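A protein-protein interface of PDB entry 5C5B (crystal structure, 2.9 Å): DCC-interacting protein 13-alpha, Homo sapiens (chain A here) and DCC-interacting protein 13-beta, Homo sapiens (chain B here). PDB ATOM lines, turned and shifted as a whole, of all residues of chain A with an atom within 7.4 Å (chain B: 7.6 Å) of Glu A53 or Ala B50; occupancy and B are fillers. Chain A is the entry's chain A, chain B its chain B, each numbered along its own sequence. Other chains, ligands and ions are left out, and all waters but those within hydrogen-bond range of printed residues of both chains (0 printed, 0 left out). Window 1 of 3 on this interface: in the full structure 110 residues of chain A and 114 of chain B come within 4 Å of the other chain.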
ATOM      1  N   ILE A  47     -11.115 -21.129  15.454  1.00  0.00           N
ATOM      2  CA  ILE A  47     -10.725 -20.118  16.437  1.00  0.00           C
ATOM      3  C   ILE A  47     -10.540 -20.738  17.825  1.00  0.00           C
ATOM      4  O   ILE A  47      -9.543 -20.483  18.514  1.00  0.00           O
ATOM      5  CB  ILE A  47     -11.772 -18.987  16.527  1.00  0.00           C
ATOM      6  CG1 ILE A  47     -11.873 -18.241  15.192  1.00  0.00           C
ATOM      7  CG2 ILE A  47     -11.438 -18.032  17.666  1.00  0.00           C
ATOM      8  CD1 ILE A  47     -10.877 -17.113  15.038  1.00  0.00           C
ATOM      9  N   TYR A  48     -11.504 -21.566  18.213  1.00  0.00           N
ATOM     10  CA  TYR A  48     -11.511 -22.214  19.522  1.00  0.00           C
ATOM     11  C   TYR A  48     -10.271 -23.088  19.728  1.00  0.00           C
ATOM     12  O   TYR A  48      -9.547 -22.954  20.731  1.00  0.00           O
ATOM     13  CB  TYR A  48     -12.787 -23.049  19.667  1.00  0.00           C
ATOM     14  CG  TYR A  48     -12.966 -23.709  21.011  1.00  0.00           C
ATOM     15  CD1 TYR A  48     -13.114 -22.951  22.164  1.00  0.00           C
ATOM     16  CD2 TYR A  48     -13.004 -25.093  21.127  1.00  0.00           C
ATOM     17  CE1 TYR A  48     -13.282 -23.550  23.394  1.00  0.00           C
ATOM     18  CE2 TYR A  48     -13.173 -25.703  22.354  1.00  0.00           C
ATOM     19  CZ  TYR A  48     -13.312 -24.927  23.485  1.00  0.00           C
ATOM     20  OH  TYR A  48     -13.481 -25.527  24.712  1.00  0.00           O
ATOM     21  N   ASP A  49     -10.027 -23.970  18.761  1.00  0.00           N
ATOM     22  CA  ASP A  49      -8.864 -24.849  18.790  1.00  0.00           C
ATOM     23  C   ASP A  49      -7.571 -24.049  18.833  1.00  0.00           C
ATOM     24  O   ASP A  49      -6.628 -24.419  19.532  1.00  0.00           O
ATOM     25  CB  ASP A  49      -8.857 -25.780  17.574  1.00  0.00           C
ATOM     26  CG  ASP A  49      -9.766 -26.978  17.752  1.00  0.00           C
ATOM     27  OD1 ASP A  49     -10.281 -27.175  18.873  1.00  0.00           O
ATOM     28  OD2 ASP A  49      -9.959 -27.729  16.772  1.00  0.00           O
ATOM     29  N   ALA A  50      -7.532 -22.953  18.081  1.00  0.00           N
ATOM     30  CA  ALA A  50      -6.367 -22.077  18.079  1.00  0.00           C
ATOM     31  C   ALA A  50      -6.088 -21.506  19.472  1.00  0.00           C
ATOM     32  O   ALA A  50      -4.952 -21.541  19.948  1.00  0.00           O
ATOM     33  CB  ALA A  50      -6.555 -20.957  17.072  1.00  0.00           C
ATOM     34  N   GLN A  51      -7.129 -20.983  20.120  1.00  0.00           N
ATOM     35  CA  GLN A  51      -6.987 -20.400  21.455  1.00  0.00           C
ATOM     36  C   GLN A  51      -6.498 -21.435  22.475  1.00  0.00           C
ATOM     37  O   GLN A  51      -5.523 -21.194  23.219  1.00  0.00           O
ATOM     38  CB  GLN A  51      -8.320 -19.794  21.907  1.00  0.00           C
ATOM     39  CG  GLN A  51      -8.246 -18.978  23.189  1.00  0.00           C
ATOM     40  CD  GLN A  51      -7.363 -17.751  23.060  1.00  0.00           C
ATOM     41  OE1 GLN A  51      -6.647 -17.389  23.993  1.00  0.00           O
ATOM     42  NE2 GLN A  51      -7.420 -17.098  21.906  1.00  0.00           N
ATOM     43  N   ASN A  52      -7.171 -22.587  22.503  1.00  0.00           N
ATOM     44  CA  ASN A  52      -6.739 -23.691  23.363  1.00  0.00           C
ATOM     45  C   ASN A  52      -5.281 -24.068  23.116  1.00  0.00           C
ATOM     46  O   ASN A  52      -4.517 -24.296  24.060  1.00  0.00           O
ATOM     47  CB  ASN A  52      -7.631 -24.917  23.161  1.00  0.00           C
ATOM     48  CG  ASN A  52      -8.914 -24.844  23.963  1.00  0.00           C
ATOM     49  OD1 ASN A  52      -8.923 -24.365  25.097  1.00  0.00           O
ATOM     50  ND2 ASN A  52     -10.005 -25.326  23.381  1.00  0.00           N
ATOM     51  N   GLU A  53      -4.903 -24.116  21.843  1.00  0.00           N
ATOM     52  CA  GLU A  53      -3.537 -24.446  21.460  1.00  0.00           C
ATOM     53  C   GLU A  53      -2.550 -23.418  22.006  1.00  0.00           C
ATOM     54  O   GLU A  53      -1.458 -23.775  22.456  1.00  0.00           O
ATOM     55  CB  GLU A  53      -3.417 -24.538  19.937  1.00  0.00           C
ATOM     56  CG  GLU A  53      -2.059 -25.012  19.450  1.00  0.00           C
ATOM     57  CD  GLU A  53      -1.497 -26.141  20.293  1.00  0.00           C
ATOM     58  OE1 GLU A  53      -2.191 -27.168  20.458  1.00  0.00           O
ATOM     59  OE2 GLU A  53      -0.363 -25.997  20.796  1.00  0.00           O
ATOM     60  N   LEU A  54      -2.938 -22.146  21.966  1.00  0.00           N
ATOM     61  CA  LEU A  54      -2.121 -21.080  22.540  1.00  0.00           C
ATOM     62  C   LEU A  54      -1.877 -21.302  24.029  1.00  0.00           C
ATOM     63  O   LEU A  54      -0.723 -21.307  24.485  1.00  0.00           O
ATOM     64  CB  LEU A  54      -2.780 -19.716  22.315  1.00  0.00           C
ATOM     65  CG  LEU A  54      -2.614 -19.097  20.927  1.00  0.00           C
ATOM     66  CD1 LEU A  54      -3.505 -17.880  20.777  1.00  0.00           C
ATOM     67  CD2 LEU A  54      -1.158 -18.722  20.696  1.00  0.00           C
ATOM     68  N   SER A  55      -2.960 -21.494  24.782  1.00  0.00           N
ATOM     69  CA  SER A  55      -2.830 -21.715  26.224  1.00  0.00           C
ATOM     70  C   SER A  55      -1.939 -22.923  26.523  1.00  0.00           C
ATOM     71  O   SER A  55      -1.057 -22.868  27.391  1.00  0.00           O
ATOM     72  CB  SER A  55      -4.204 -21.905  26.870  1.00  0.00           C
ATOM     73  OG  SER A  55      -4.865 -23.038  26.340  1.00  0.00           O
ATOM     74  N   ALA A  56      -2.165 -24.002  25.778  1.00  0.00           N
ATOM     75  CA  ALA A  56      -1.385 -25.227  25.929  1.00  0.00           C
ATOM     76  C   ALA A  56       0.108 -24.992  25.699  1.00  0.00           C
ATOM     77  O   ALA A  56       0.938 -25.389  26.520  1.00  0.00           O
ATOM     78  CB  ALA A  56      -1.902 -26.297  24.980  1.00  0.00           C
ATOM     79  N   ALA A  57       0.441 -24.351  24.581  1.00  0.00           N
ATOM     80  CA  ALA A  57       1.833 -24.084  24.227  1.00  0.00           C
ATOM     81  C   ALA A  57       2.517 -23.227  25.289  1.00  0.00           C
ATOM     82  O   ALA A  57       3.657 -23.500  25.693  1.00  0.00           O
ATOM     83  CB  ALA A  57       1.911 -23.409  22.866  1.00  0.00           C
ATOM     84  N   THR A  58       1.811 -22.191  25.736  1.00  0.00           N
ATOM     85  CA  THR A  58       2.330 -21.305  26.773  1.00  0.00           C
ATOM     86  C   THR A  58       2.657 -22.088  28.048  1.00  0.00           C
ATOM     87  O   THR A  58       3.773 -21.998  28.594  1.00  0.00           O
ATOM     88  CB  THR A  58       1.315 -20.190  27.099  1.00  0.00           C
ATOM     89  OG1 THR A  58       0.705 -19.727  25.888  1.00  0.00           O
ATOM     90  CG2 THR A  58       1.996 -19.029  27.792  1.00  0.00           C
ATOM     91  N   HIS A  59       1.685 -22.878  28.499  1.00  0.00           N
ATOM     92  CA  HIS A  59       1.860 -23.710  29.685  1.00  0.00           C
ATOM     93  C   HIS A  59       3.054 -24.656  29.545  1.00  0.00           C
ATOM     94  O   HIS A  59       3.850 -24.815  30.478  1.00  0.00           O
ATOM     95  CB  HIS A  59       0.589 -24.516  29.963  1.00  0.00           C
ATOM     96  CG  HIS A  59       0.640 -25.299  31.237  1.00  0.00           C
ATOM     97  ND1 HIS A  59       0.544 -24.709  32.478  1.00  0.00           N
ATOM     98  CD2 HIS A  59       0.782 -26.627  31.462  1.00  0.00           C
ATOM     99  CE1 HIS A  59       0.621 -25.639  33.413  1.00  0.00           C
ATOM    100  NE2 HIS A  59       0.766 -26.812  32.823  1.00  0.00           N
ATOM    101  N   LEU A  60       3.172 -25.277  28.375  1.00  0.00           N
ATOM    102  CA  LEU A  60       4.245 -26.229  28.105  1.00  0.00           C
ATOM    103  C   LEU A  60       5.622 -25.574  28.201  1.00  0.00           C
ATOM    104  O   LEU A  60       6.545 -26.112  28.840  1.00  0.00           O
ATOM    105  CB  LEU A  60       4.057 -26.852  26.721  1.00  0.00           C
ATOM    106  CG  LEU A  60       4.278 -28.360  26.616  1.00  0.00           C
ATOM    107  CD1 LEU A  60       3.070 -29.111  27.158  1.00  0.00           C
ATOM    108  CD2 LEU A  60       4.570 -28.763  25.180  1.00  0.00           C
ATOM    109  N   HIS A 100      -5.054 -16.868  28.321  1.00  0.00           N
ATOM    110  CA  HIS A 100      -5.507 -17.641  27.167  1.00  0.00           C
ATOM    111  C   HIS A 100      -6.514 -18.721  27.566  1.00  0.00           C
ATOM    112  O   HIS A 100      -7.442 -19.024  26.816  1.00  0.00           O
ATOM    113  CB  HIS A 100      -4.318 -18.277  26.445  1.00  0.00           C
ATOM    114  CG  HIS A 100      -3.500 -17.306  25.651  1.00  0.00           C
ATOM    115  ND1 HIS A 100      -4.007 -16.614  24.574  1.00  0.00           N
ATOM    116  CD2 HIS A 100      -2.207 -16.922  25.772  1.00  0.00           C
ATOM    117  CE1 HIS A 100      -3.063 -15.838  24.068  1.00  0.00           C
ATOM    118  NE2 HIS A 100      -1.962 -16.007  24.777  1.00  0.00           N
ATOM    119  N   SER A 104     -10.332 -19.099  26.497  1.00  0.00           N
ATOM    120  CA  SER A 104     -10.792 -20.350  25.899  1.00  0.00           C
ATOM    121  C   SER A 104     -12.133 -20.781  26.478  1.00  0.00           C
ATOM    122  O   SER A 104     -13.053 -21.129  25.737  1.00  0.00           O
ATOM    123  CB  SER A 104      -9.760 -21.461  26.097  1.00  0.00           C
ATOM    124  OG  SER A 104      -8.722 -21.378  25.138  1.00  0.00           O
ATOM    125  N   MET B  44       9.445 -22.988  21.743  1.00  0.00           N
ATOM    126  CA  MET B  44       9.287 -21.703  21.068  1.00  0.00           C
ATOM    127  C   MET B  44       8.573 -21.854  19.734  1.00  0.00           C
ATOM    128  O   MET B  44       7.631 -21.119  19.441  1.00  0.00           O
ATOM    129  CB  MET B  44      10.645 -21.031  20.857  1.00  0.00           C
ATOM    130  CG  MET B  44      11.373 -20.652  22.140  1.00  0.00           C
ATOM    131  SD  MET B  44      10.399 -19.632  23.262  1.00  0.00           S
ATOM    132  CE  MET B  44       9.894 -20.845  24.477  1.00  0.00           C
ATOM    133  N   GLN B  45       9.035 -22.801  18.924  1.00  0.00           N
ATOM    134  CA  GLN B  45       8.417 -23.052  17.627  1.00  0.00           C
ATOM    135  C   GLN B  45       6.948 -23.447  17.768  1.00  0.00           C
ATOM    136  O   GLN B  45       6.129 -23.114  16.908  1.00  0.00           O
ATOM    137  CB  GLN B  45       9.195 -24.114  16.851  1.00  0.00           C
ATOM    138  CG  GLN B  45      10.328 -23.533  16.012  1.00  0.00           C
ATOM    139  CD  GLN B  45      11.316 -24.584  15.554  1.00  0.00           C
ATOM    140  OE1 GLN B  45      11.143 -25.771  15.822  1.00  0.00           O
ATOM    141  NE2 GLN B  45      12.344 -24.154  14.829  1.00  0.00           N
ATOM    142  N   ARG B  46       6.606 -24.146  18.848  1.00  0.00           N
ATOM    143  CA  ARG B  46       5.201 -24.469  19.084  1.00  0.00           C
ATOM    144  C   ARG B  46       4.392 -23.216  19.432  1.00  0.00           C
ATOM    145  O   ARG B  46       3.263 -23.050  18.959  1.00  0.00           O
ATOM    146  CB  ARG B  46       5.058 -25.516  20.189  1.00  0.00           C
ATOM    147  CG  ARG B  46       4.945 -26.936  19.664  1.00  0.00           C
ATOM    148  CD  ARG B  46       4.300 -27.861  20.681  1.00  0.00           C
ATOM    149  NE  ARG B  46       3.024 -27.338  21.161  1.00  0.00           N
ATOM    150  CZ  ARG B  46       2.250 -27.956  22.049  1.00  0.00           C
ATOM    151  NH1 ARG B  46       2.615 -29.128  22.546  1.00  0.00           N
ATOM    152  NH2 ARG B  46       1.106 -27.405  22.432  1.00  0.00           N
ATOM    153  N   VAL B  47       4.969 -22.331  20.242  1.00  0.00           N
ATOM    154  CA  VAL B  47       4.292 -21.076  20.574  1.00  0.00           C
ATOM    155  C   VAL B  47       4.048 -20.220  19.323  1.00  0.00           C
ATOM    156  O   VAL B  47       2.923 -19.761  19.068  1.00  0.00           O
ATOM    157  CB  VAL B  47       5.098 -20.255  21.601  1.00  0.00           C
ATOM    158  CG1 VAL B  47       4.542 -18.842  21.708  1.00  0.00           C
ATOM    159  CG2 VAL B  47       5.082 -20.941  22.959  1.00  0.00           C
ATOM    160  N   TYR B  48       5.106 -20.025  18.541  1.00  0.00           N
ATOM    161  CA  TYR B  48       5.020 -19.284  17.287  1.00  0.00           C
ATOM    162  C   TYR B  48       3.995 -19.892  16.335  1.00  0.00           C
ATOM    163  O   TYR B  48       3.170 -19.176  15.762  1.00  0.00           O
ATOM    164  CB  TYR B  48       6.389 -19.227  16.606  1.00  0.00           C
ATOM    165  CG  TYR B  48       6.320 -18.799  15.157  1.00  0.00           C
ATOM    166  CD1 TYR B  48       6.035 -17.484  14.811  1.00  0.00           C
ATOM    167  CD2 TYR B  48       6.532 -19.715  14.134  1.00  0.00           C
ATOM    168  CE1 TYR B  48       5.967 -17.094  13.485  1.00  0.00           C
ATOM    169  CE2 TYR B  48       6.466 -19.334  12.808  1.00  0.00           C
ATOM    170  CZ  TYR B  48       6.183 -18.023  12.489  1.00  0.00           C
ATOM    171  OH  TYR B  48       6.118 -17.643  11.168  1.00  0.00           O
ATOM    172  N   GLY B  49       4.057 -21.209  16.168  1.00  0.00           N
ATOM    173  CA  GLY B  49       3.109 -21.919  15.328  1.00  0.00           C
ATOM    174  C   GLY B  49       1.676 -21.689  15.768  1.00  0.00           C
ATOM    175  O   GLY B  49       0.784 -21.483  14.941  1.00  0.00           O
ATOM    176  N   ALA B  50       1.462 -21.710  17.080  1.00  0.00           N
ATOM    177  CA  ALA B  50       0.137 -21.488  17.645  1.00  0.00           C
ATOM    178  C   ALA B  50      -0.372 -20.085  17.318  1.00  0.00           C
ATOM    179  O   ALA B  50      -1.518 -19.914  16.883  1.00  0.00           O
ATOM    180  CB  ALA B  50       0.162 -21.709  19.150  1.00  0.00           C
ATOM    181  N   GLN B  51       0.487 -19.087  17.517  1.00  0.00           N
ATOM    182  CA  GLN B  51       0.128 -17.708  17.194  1.00  0.00           C
ATOM    183  C   GLN B  51      -0.243 -17.579  15.716  1.00  0.00           C
ATOM    184  O   GLN B  51      -1.253 -16.959  15.358  1.00  0.00           O
ATOM    185  CB  GLN B  51       1.279 -16.760  17.532  1.00  0.00           C
ATOM    186  CG  GLN B  51       0.842 -15.331  17.780  1.00  0.00           C
ATOM    187  CD  GLN B  51      -0.024 -15.203  19.016  1.00  0.00           C
ATOM    188  OE1 GLN B  51      -1.108 -14.621  18.974  1.00  0.00           O
ATOM    189  NE2 GLN B  51       0.452 -15.750  20.129  1.00  0.00           N
ATOM    190  N   ASN B  52       0.582 -18.180  14.866  1.00  0.00           N
ATOM    191  CA  ASN B  52       0.339 -18.203  13.429  1.00  0.00           C
ATOM    192  C   ASN B  52      -1.005 -18.814  13.038  1.00  0.00           C
ATOM    193  O   ASN B  52      -1.735 -18.273  12.195  1.00  0.00           O
ATOM    194  CB  ASN B  52       1.464 -18.969  12.730  1.00  0.00           C
ATOM    195  CG  ASN B  52       1.435 -18.808  11.226  1.00  0.00           C
ATOM    196  OD1 ASN B  52       1.650 -17.716  10.701  1.00  0.00           O
ATOM    197  ND2 ASN B  52       1.164 -19.902  10.521  1.00  0.00           N
ATOM    198  N   GLU B  53      -1.342 -19.943  13.653  1.00  0.00           N
ATOM    199  CA  GLU B  53      -2.597 -20.598  13.323  1.00  0.00           C
ATOM    200  C   GLU B  53      -3.773 -19.771  13.854  1.00  0.00           C
ATOM    201  O   GLU B  53      -4.869 -19.821  13.296  1.00  0.00           O
ATOM    202  CB  GLU B  53      -2.636 -22.023  13.874  1.00  0.00           C
ATOM    203  CG  GLU B  53      -3.814 -22.820  13.353  1.00  0.00           C
ATOM    204  CD  GLU B  53      -3.540 -23.359  11.958  1.00  0.00           C
ATOM    205  OE1 GLU B  53      -2.368 -23.696  11.683  1.00  0.00           O
ATOM    206  OE2 GLU B  53      -4.478 -23.423  11.135  1.00  0.00           O
ATOM    207  N   MET B  54      -3.556 -19.029  14.939  1.00  0.00           N
ATOM    208  CA  MET B  54      -4.569 -18.078  15.394  1.00  0.00           C
ATOM    209  C   MET B  54      -4.786 -16.985  14.347  1.00  0.00           C
ATOM    210  O   MET B  54      -5.924 -16.553  14.103  1.00  0.00           O
ATOM    211  CB  MET B  54      -4.172 -17.452  16.732  1.00  0.00           C
ATOM    212  CG  MET B  54      -5.141 -16.381  17.225  1.00  0.00           C
ATOM    213  SD  MET B  54      -6.877 -16.884  17.222  1.00  0.00           S
ATOM    214  CE  MET B  54      -6.973 -17.846  18.727  1.00  0.00           C
ATOM    215  N   CYS B  55      -3.690 -16.539  13.737  1.00  0.00           N
ATOM    216  CA  CYS B  55      -3.768 -15.573  12.644  1.00  0.00           C
ATOM    217  C   CYS B  55      -4.637 -16.117  11.516  1.00  0.00           C
ATOM    218  O   CYS B  55      -5.592 -15.464  11.080  1.00  0.00           O
ATOM    219  CB  CYS B  55      -2.372 -15.237  12.118  1.00  0.00           C
ATOM    220  SG  CYS B  55      -1.330 -14.354  13.289  1.00  0.00           S
ATOM    221  N   LEU B  56      -4.304 -17.321  11.053  1.00  0.00           N
ATOM    222  CA  LEU B  56      -5.064 -17.966   9.983  1.00  0.00           C
ATOM    223  C   LEU B  56      -6.540 -18.130  10.345  1.00  0.00           C
ATOM    224  O   LEU B  56      -7.423 -17.924   9.509  1.00  0.00           O
ATOM    225  CB  LEU B  56      -4.464 -19.332   9.646  1.00  0.00           C
ATOM    226  CG  LEU B  56      -3.096 -19.326   8.964  1.00  0.00           C
ATOM    227  CD1 LEU B  56      -2.582 -20.745   8.770  1.00  0.00           C
ATOM    228  CD2 LEU B  56      -3.169 -18.590   7.636  1.00  0.00           C
ATOM    229  N   ALA B  57      -6.795 -18.500  11.597  1.00  0.00           N
ATOM    230  CA  ALA B  57      -8.150 -18.701  12.097  1.00  0.00           C
ATOM    231  C   ALA B  57      -8.964 -17.418  12.004  1.00  0.00           C
ATOM    232  O   ALA B  57     -10.074 -17.416  11.465  1.00  0.00           O
ATOM    233  CB  ALA B  57      -8.120 -19.206  13.530  1.00  0.00           C
ATOM    234  N   HIS B 100      -2.530  -9.985  15.914  1.00  0.00           N
ATOM    235  CA  HIS B 100      -2.008 -11.344  16.043  1.00  0.00           C
ATOM    236  C   HIS B 100      -0.820 -11.579  15.116  1.00  0.00           C
ATOM    237  O   HIS B 100       0.154 -12.231  15.494  1.00  0.00           O
ATOM    238  CB  HIS B 100      -3.102 -12.374  15.746  1.00  0.00           C
ATOM    239  CG  HIS B 100      -4.016 -12.640  16.901  1.00  0.00           C
ATOM    240  ND1 HIS B 100      -3.604 -13.297  18.040  1.00  0.00           N
ATOM    241  CD2 HIS B 100      -5.328 -12.355  17.084  1.00  0.00           C
ATOM    242  CE1 HIS B 100      -4.620 -13.395  18.881  1.00  0.00           C
ATOM    243  NE2 HIS B 100      -5.677 -12.832  18.324  1.00  0.00           N
ATOM    244  N   ALA B 104       2.973 -12.541  16.087  1.00  0.00           N
ATOM    245  CA  ALA B 104       3.621 -13.713  15.506  1.00  0.00           C
ATOM    246  C   ALA B 104       4.987 -13.357  14.925  1.00  0.00           C
ATOM    247  O   ALA B 104       5.971 -14.080  15.125  1.00  0.00           O
ATOM    248  CB  ALA B 104       2.736 -14.334  14.436  1.00  0.00           C
ATOM    249  N   LEU B 107       7.398 -12.779  17.727  1.00  0.00           N
ATOM    250  CA  LEU B 107       7.898 -14.030  18.285  1.00  0.00           C
ATOM    251  C   LEU B 107       8.974 -14.614  17.376  1.00  0.00           C
ATOM    252  O   LEU B 107      10.035 -15.038  17.840  1.00  0.00           O
ATOM    253  CB  LEU B 107       6.762 -15.043  18.462  1.00  0.00           C
ATOM    254  CG  LEU B 107       5.572 -14.685  19.356  1.00  0.00           C
ATOM    255  CD1 LEU B 107       4.561 -15.823  19.369  1.00  0.00           C
ATOM    256  CD2 LEU B 107       6.018 -14.349  20.769  1.00  0.00           C
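The side-chain carboxylate (OE2) of Glu A53 is in salt-bridge range of the guanidinium group (NH2) of Arg B46, 2.6 Å away.
A ring nitrogen (ND1) of His A100 sits at hydrogen-bond distance from the side-chain amide oxygen (OE1) of Gln A51 (2.8 Å). O of Leu A54 lies within hydrogen-bond range of OG1 of Thr A58, 2.6 Å away. SG of Cys B55 sits at hydrogen-bond distance from O of Gln B51 (3.3 Å). A ring nitrogen (ND1) of His B100 lies within hydrogen-bond range of the side-chain amide oxygen (OE1) of Gln B51 (3.0 Å).
Among the printed residues, pairs that only touch across the chains: Ile A47 with Met B54 (3.7 Å), Ile A47 with Ala B57 (3.6 Å), Ala A50 with Met B54 (3.5 Å), Gln A51 with Met B54 (3.3 Å), Glu A53 with Ala B50 (3.99 Å), Leu A54 with Ala B50 (3.6 Å), Leu A54 with Gln B51 (3.4 Å), Ala A57 with Arg B46 (3.8 Å) and Leu A60 with Arg B46 (3.3 Å).
Printed residues of chain B within 4 Å of Ile A47: Met B54 and Ala B57. Of the printed residues of chain B, Ala A50 touches Met B54 (3.5 Å). Of the printed residues of chain B, Glu A53 touches Arg B46 and Ala B50. Printed residues of chain B within 4 Å of Leu A54: Ala B50 (3.6 Å) and Gln B51 (3.4 Å). Ser A104 touches none of the printed residues of chain B. No residue of chain A comes within 4 Å of Gly B49. Of the printed residues of chain A, Ala B50 touches Glu A53 and Leu A54. Of the printed residues of chain A, Met B54 touches Ile A47 (3.7 Å), Ala A50 (3.5 Å) and Gln A51 (3.3 Å). Cys B55 touches none of the printed residues of chain A.
Hydrophobic or aromatic side chains of chain A that line the printed part of chain B: Ile A47, Ala A50, Leu A54 and Leu A60. Of the 17 printed residues of chain B, 5 touch a printed residue of chain A. Hydrophobic or aromatic side chains of chain B that line the printed part of chain A: Ala B50, Met B54 and Ala B57. Among the printed residues, 10 pairs touch across the chains.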
